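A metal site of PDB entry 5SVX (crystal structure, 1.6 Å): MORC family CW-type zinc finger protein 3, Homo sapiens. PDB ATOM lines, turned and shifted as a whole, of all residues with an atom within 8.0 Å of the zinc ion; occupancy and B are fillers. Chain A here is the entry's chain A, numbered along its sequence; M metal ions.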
ATOM      1  N   GLN A   7      15.209 -13.430   8.375  1.00  0.00           N
ATOM      2  CA  GLN A   7      14.926 -13.555   9.795  1.00  0.00           C
ATOM      3  C   GLN A   7      14.794 -15.010  10.212  1.00  0.00           C
ATOM      4  O   GLN A   7      14.112 -15.802   9.577  1.00  0.00           O
ATOM      5  CB  GLN A   7      13.643 -12.812  10.166  1.00  0.00           C
ATOM      6  CG  GLN A   7      13.400 -12.798  11.659  1.00  0.00           C
ATOM      7  CD  GLN A   7      12.209 -11.951  12.056  1.00  0.00           C
ATOM      8  OE1 GLN A   7      11.095 -12.172  11.583  1.00  0.00           O
ATOM      9  NE2 GLN A   7      12.436 -10.998  12.936  1.00  0.00           N
ATOM     10  N   CYS A   8      15.476 -15.353  11.304  1.00  0.00           N
ATOM     11  CA  CYS A   8      15.312 -16.666  11.913  1.00  0.00           C
ATOM     12  C   CYS A   8      13.914 -16.809  12.503  1.00  0.00           C
ATOM     13  O   CYS A   8      13.484 -15.988  13.302  1.00  0.00           O
ATOM     14  CB  CYS A   8      16.359 -16.886  13.000  1.00  0.00           C
ATOM     15  SG  CYS A   8      16.171 -18.481  13.825  1.00  0.00           S
ATOM     16  N   ASP A   9      13.215 -17.870  12.132  1.00  0.00           N
ATOM     17  CA  ASP A   9      11.843 -18.042  12.586  1.00  0.00           C
ATOM     18  C   ASP A   9      11.764 -18.607  14.004  1.00  0.00           C
ATOM     19  O   ASP A   9      10.667 -18.727  14.561  1.00  0.00           O
ATOM     20  CB  ASP A   9      11.080 -18.913  11.586  1.00  0.00           C
ATOM     21  CG  ASP A   9      10.773 -18.161  10.289  1.00  0.00           C
ATOM     22  OD1 ASP A   9      10.375 -16.988  10.371  1.00  0.00           O
ATOM     23  OD2 ASP A   9      10.952 -18.734   9.185  1.00  0.00           O
ATOM     24  N   ALA A  10      12.907 -18.920  14.599  1.00  0.00           N
ATOM     25  CA  ALA A  10      12.949 -19.348  16.004  1.00  0.00           C
ATOM     26  C   ALA A  10      13.310 -18.202  16.940  1.00  0.00           C
ATOM     27  O   ALA A  10      12.597 -17.950  17.910  1.00  0.00           O
ATOM     28  CB  ALA A  10      13.945 -20.495  16.177  1.00  0.00           C
ATOM     29  N   CYS A  11      14.404 -17.505  16.647  1.00  0.00           N
ATOM     30  CA  CYS A  11      14.921 -16.486  17.574  1.00  0.00           C
ATOM     31  C   CYS A  11      14.663 -15.047  17.106  1.00  0.00           C
ATOM     32  O   CYS A  11      14.889 -14.109  17.867  1.00  0.00           O
ATOM     33  CB  CYS A  11      16.425 -16.705  17.797  1.00  0.00           C
ATOM     34  SG  CYS A  11      17.520 -16.116  16.488  1.00  0.00           S
ATOM     35  N   LEU A  12      14.192 -14.905  15.865  1.00  0.00           N
ATOM     36  CA  LEU A  12      13.797 -13.620  15.286  1.00  0.00           C
ATOM     37  C   LEU A  12      14.972 -12.673  15.005  1.00  0.00           C
ATOM     38  O   LEU A  12      14.771 -11.503  14.672  1.00  0.00           O
ATOM     39  CB  LEU A  12      12.751 -12.925  16.173  1.00  0.00           C
ATOM     40  CG  LEU A  12      11.476 -13.729  16.417  1.00  0.00           C
ATOM     41  CD1 LEU A  12      10.513 -12.914  17.277  1.00  0.00           C
ATOM     42  CD2 LEU A  12      10.811 -14.134  15.101  1.00  0.00           C
ATOM     43  N   LYS A  13      16.195 -13.182  15.102  1.00  0.00           N
ATOM     44  CA  LYS A  13      17.351 -12.406  14.663  1.00  0.00           C
ATOM     45  C   LYS A  13      17.418 -12.355  13.139  1.00  0.00           C
ATOM     46  O   LYS A  13      17.071 -13.310  12.449  1.00  0.00           O
ATOM     47  CB  LYS A  13      18.655 -12.975  15.201  1.00  0.00           C
ATOM     48  CG  LYS A  13      18.819 -12.847  16.697  1.00  0.00           C
ATOM     49  CD  LYS A  13      20.170 -13.383  17.137  1.00  0.00           C
ATOM     50  CE  LYS A  13      20.321 -13.369  18.647  1.00  0.00           C
ATOM     51  NZ  LYS A  13      19.370 -14.298  19.307  1.00  0.00           N
ATOM     52  N   TRP A  14      17.891 -11.223  12.634  1.00  0.00           N
ATOM     53  CA  TRP A  14      18.161 -11.065  11.218  1.00  0.00           C
ATOM     54  C   TRP A  14      19.593 -11.466  10.896  1.00  0.00           C
ATOM     55  O   TRP A  14      20.538 -11.064  11.587  1.00  0.00           O
ATOM     56  CB  TRP A  14      17.916  -9.619  10.807  1.00  0.00           C
ATOM     57  CG  TRP A  14      16.478  -9.234  10.891  1.00  0.00           C
ATOM     58  CD1 TRP A  14      15.829  -8.694  11.973  1.00  0.00           C
ATOM     59  CD2 TRP A  14      15.502  -9.355   9.864  1.00  0.00           C
ATOM     60  NE1 TRP A  14      14.510  -8.476  11.670  1.00  0.00           N
ATOM     61  CE2 TRP A  14      14.282  -8.875  10.373  1.00  0.00           C
ATOM     62  CE3 TRP A  14      15.530  -9.835   8.551  1.00  0.00           C
ATOM     63  CZ2 TRP A  14      13.116  -8.850   9.624  1.00  0.00           C
ATOM     64  CZ3 TRP A  14      14.378  -9.809   7.807  1.00  0.00           C
ATOM     65  CH2 TRP A  14      13.188  -9.320   8.336  1.00  0.00           C
ATOM     66  N   ARG A  15      19.739 -12.271   9.839  1.00  0.00           N
ATOM     67  CA  ARG A  15      21.033 -12.765   9.387  1.00  0.00           C
ATOM     68  C   ARG A  15      21.310 -12.322   7.972  1.00  0.00           C
ATOM     69  O   ARG A  15      20.474 -12.476   7.090  1.00  0.00           O
ATOM     70  CB  ARG A  15      21.086 -14.297   9.465  1.00  0.00           C
ATOM     71  CG  ARG A  15      20.796 -14.858  10.840  1.00  0.00           C
ATOM     72  CD  ARG A  15      21.753 -14.321  11.881  1.00  0.00           C
ATOM     73  NE  ARG A  15      21.718 -15.127  13.099  1.00  0.00           N
ATOM     74  CZ  ARG A  15      22.301 -14.797  14.240  1.00  0.00           C
ATOM     75  NH1 ARG A  15      22.969 -13.657  14.346  1.00  0.00           N
ATOM     76  NH2 ARG A  15      22.210 -15.595  15.286  1.00  0.00           N
ATOM     77  N   TRP A  28      12.885 -20.496   7.807  1.00  0.00           N
ATOM     78  CA  TRP A  28      14.344 -20.387   7.826  1.00  0.00           C
ATOM     79  C   TRP A  28      14.808 -20.193   9.255  1.00  0.00           C
ATOM     80  O   TRP A  28      14.188 -19.455  10.029  1.00  0.00           O
ATOM     81  CB  TRP A  28      14.808 -19.226   6.945  1.00  0.00           C
ATOM     82  CG  TRP A  28      16.288 -19.218   6.694  1.00  0.00           C
ATOM     83  CD1 TRP A  28      16.927 -19.738   5.614  1.00  0.00           C
ATOM     84  CD2 TRP A  28      17.299 -18.634   7.526  1.00  0.00           C
ATOM     85  NE1 TRP A  28      18.277 -19.531   5.723  1.00  0.00           N
ATOM     86  CE2 TRP A  28      18.537 -18.864   6.886  1.00  0.00           C
ATOM     87  CE3 TRP A  28      17.277 -17.963   8.745  1.00  0.00           C
ATOM     88  CZ2 TRP A  28      19.740 -18.440   7.437  1.00  0.00           C
ATOM     89  CZ3 TRP A  28      18.482 -17.537   9.286  1.00  0.00           C
ATOM     90  CH2 TRP A  28      19.690 -17.774   8.626  1.00  0.00           C
ATOM     91  N   TYR A  29      15.917 -20.853   9.607  1.00  0.00           N
ATOM     92  CA  TYR A  29      16.495 -20.768  10.935  1.00  0.00           C
ATOM     93  C   TYR A  29      18.005 -20.555  10.864  1.00  0.00           C
ATOM     94  O   TYR A  29      18.633 -20.918   9.870  1.00  0.00           O
ATOM     95  CB  TYR A  29      16.217 -22.044  11.724  1.00  0.00           C
ATOM     96  CG  TYR A  29      14.776 -22.448  11.749  1.00  0.00           C
ATOM     97  CD1 TYR A  29      13.915 -21.964  12.711  1.00  0.00           C
ATOM     98  CD2 TYR A  29      14.273 -23.323  10.794  1.00  0.00           C
ATOM     99  CE1 TYR A  29      12.583 -22.329  12.731  1.00  0.00           C
ATOM    100  CE2 TYR A  29      12.935 -23.695  10.811  1.00  0.00           C
ATOM    101  CZ  TYR A  29      12.107 -23.200  11.784  1.00  0.00           C
ATOM    102  OH  TYR A  29      10.774 -23.565  11.804  1.00  0.00           O
ATOM    103  N   CYS A  30      18.563 -20.005  11.931  1.00  0.00           N
ATOM    104  CA  CYS A  30      19.993 -19.765  12.004  1.00  0.00           C
ATOM    105  C   CYS A  30      20.795 -21.007  11.642  1.00  0.00           C
ATOM    106  O   CYS A  30      21.823 -20.922  10.975  1.00  0.00           O
ATOM    107  CB  CYS A  30      20.385 -19.309  13.409  1.00  0.00           C
ATOM    108  SG  CYS A  30      19.786 -17.684  13.876  1.00  0.00           S
ATOM    109  N   SER A  31      20.292 -22.174  12.037  1.00  0.00           N
ATOM    110  CA  SER A  31      20.990 -23.422  11.784  1.00  0.00           C
ATOM    111  C   SER A  31      21.203 -23.702  10.289  1.00  0.00           C
ATOM    112  O   SER A  31      22.035 -24.532   9.930  1.00  0.00           O
ATOM    113  CB  SER A  31      20.230 -24.581  12.431  1.00  0.00           C
ATOM    114  OG  SER A  31      18.870 -24.568  12.063  1.00  0.00           O
ATOM    115  N   PHE A  38      27.327 -17.601  12.098  1.00  0.00           N
ATOM    116  CA  PHE A  38      25.997 -17.144  12.479  1.00  0.00           C
ATOM    117  C   PHE A  38      24.965 -18.263  12.347  1.00  0.00           C
ATOM    118  O   PHE A  38      23.822 -18.027  11.936  1.00  0.00           O
ATOM    119  CB  PHE A  38      25.596 -15.947  11.615  1.00  0.00           C
ATOM    120  CG  PHE A  38      26.499 -14.761  11.791  1.00  0.00           C
ATOM    121  CD1 PHE A  38      26.336 -13.895  12.858  1.00  0.00           C
ATOM    122  CD2 PHE A  38      27.521 -14.513  10.895  1.00  0.00           C
ATOM    123  CE1 PHE A  38      27.168 -12.815  13.036  1.00  0.00           C
ATOM    124  CE2 PHE A  38      28.358 -13.429  11.054  1.00  0.00           C
ATOM    125  CZ  PHE A  38      28.185 -12.574  12.136  1.00  0.00           C
ATOM    126  N   ARG A  39      25.377 -19.466  12.727  1.00  0.00           N
ATOM    127  CA  ARG A  39      24.575 -20.671  12.541  1.00  0.00           C
ATOM    128  C   ARG A  39      23.928 -21.144  13.844  1.00  0.00           C
ATOM    129  O   ARG A  39      23.325 -22.215  13.896  1.00  0.00           O
ATOM    130  CB  ARG A  39      25.476 -21.761  11.953  1.00  0.00           C
ATOM    131  CG  ARG A  39      24.757 -22.871  11.228  1.00  0.00           C
ATOM    132  CD  ARG A  39      25.769 -23.807  10.607  1.00  0.00           C
ATOM    133  NE  ARG A  39      26.259 -23.339   9.316  1.00  0.00           N
ATOM    134  CZ  ARG A  39      27.275 -23.884   8.666  1.00  0.00           C
ATOM    135  NH1 ARG A  39      27.949 -24.899   9.197  1.00  0.00           N
ATOM    136  NH2 ARG A  39      27.643 -23.396   7.485  1.00  0.00           N
ATOM    137  N   ASN A  40      24.043 -20.332  14.886  1.00  0.00           N
ATOM    138  CA  ASN A  40      23.473 -20.625  16.185  1.00  0.00           C
ATOM    139  C   ASN A  40      22.646 -19.436  16.655  1.00  0.00           C
ATOM    140  O   ASN A  40      23.089 -18.300  16.544  1.00  0.00           O
ATOM    141  CB  ASN A  40      24.582 -20.954  17.200  1.00  0.00           C
ATOM    142  CG  ASN A  40      24.042 -21.552  18.481  1.00  0.00           C
ATOM    143  OD1 ASN A  40      23.341 -20.884  19.250  1.00  0.00           O
ATOM    144  ND2 ASN A  40      24.365 -22.818  18.730  1.00  0.00           N
ATOM    145  N   CYS A  41      21.445 -19.694  17.166  1.00  0.00           N
ATOM    146  CA  CYS A  41      20.554 -18.611  17.565  1.00  0.00           C
ATOM    147  C   CYS A  41      21.131 -17.739  18.676  1.00  0.00           C
ATOM    148  O   CYS A  41      20.663 -16.624  18.896  1.00  0.00           O
ATOM    149  CB  CYS A  41      19.210 -19.187  18.021  1.00  0.00           C
ATOM    150  SG  CYS A  41      18.185 -19.874  16.698  1.00  0.00           S
ATOM    151  N   GLU A  42      22.150 -18.215  19.382  1.00  0.00           N
ATOM    152  CA  GLU A  42      22.702 -17.440  20.487  1.00  0.00           C
ATOM    153  C   GLU A  42      23.646 -16.337  20.022  1.00  0.00           C
ATOM    154  O   GLU A  42      23.916 -15.394  20.753  1.00  0.00           O
ATOM    155  CB  GLU A  42      23.414 -18.358  21.482  1.00  0.00           C
ATOM    156  CG  GLU A  42      22.454 -19.179  22.342  1.00  0.00           C
ATOM    157  CD  GLU A  42      22.109 -18.503  23.659  1.00  0.00           C
ATOM    158  OE1 GLU A  42      21.185 -17.648  23.682  1.00  0.00           O
ATOM    159  OE2 GLU A  42      22.757 -18.816  24.675  1.00  0.00           O
ATOM    160  N   VAL A  43      24.130 -16.438  18.784  1.00  0.00           N
ATOM    161  CA  VAL A  43      25.055 -15.429  18.262  1.00  0.00           C
ATOM    162  C   VAL A  43      24.295 -14.118  18.027  1.00  0.00           C
ATOM    163  O   VAL A  43      23.265 -14.107  17.353  1.00  0.00           O
ATOM    164  CB  VAL A  43      25.718 -15.896  16.947  1.00  0.00           C
ATOM    165  CG1 VAL A  43      26.647 -14.822  16.388  1.00  0.00           C
ATOM    166  CG2 VAL A  43      26.478 -17.192  17.175  1.00  0.00           C
HETATM  167 ZN    ZN M   1      17.962 -18.070  15.285  1.00  0.00          ZN
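The backbone carbonyl oxygen (O) of Cys 41 lies within hydrogen-bond range of the side-chain amino group (NZ) of Lys 13 (2.7 Å). The guanidinium group (NE) of Arg 15 sits close to the side-chain sulfur (SG) of Cys 30 (3.3 Å). The side-chain sulfur (SG) of Cys 8 sits close to the backbone NH (N) of Ala 10, 3.4 Å away. N of Cys 8 lies within hydrogen-bond range of O of Lys 13 (2.8 Å). The side-chain sulfur of Cys 11 sits close to the backbone NH of Lys 13 (3.5 Å).
Of the 19 residues printed, 4 come within 4 Å of the zinc ion. The nearest printed residue that does not touch the zinc ion is Ala 10 (4.8 Å).
The zinc ion is bound by SG of Cys 41 (2.3 Å). SG of Cys 11 binds the zinc ion, at 2.3 Å. The side-chain sulfur (SG) of Cys 30 binds the zinc ion (2.3 Å). The zinc ion is bound by SG of Cys 8 (2.3 Å). The zinc ion has four donor atoms within binding distance.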
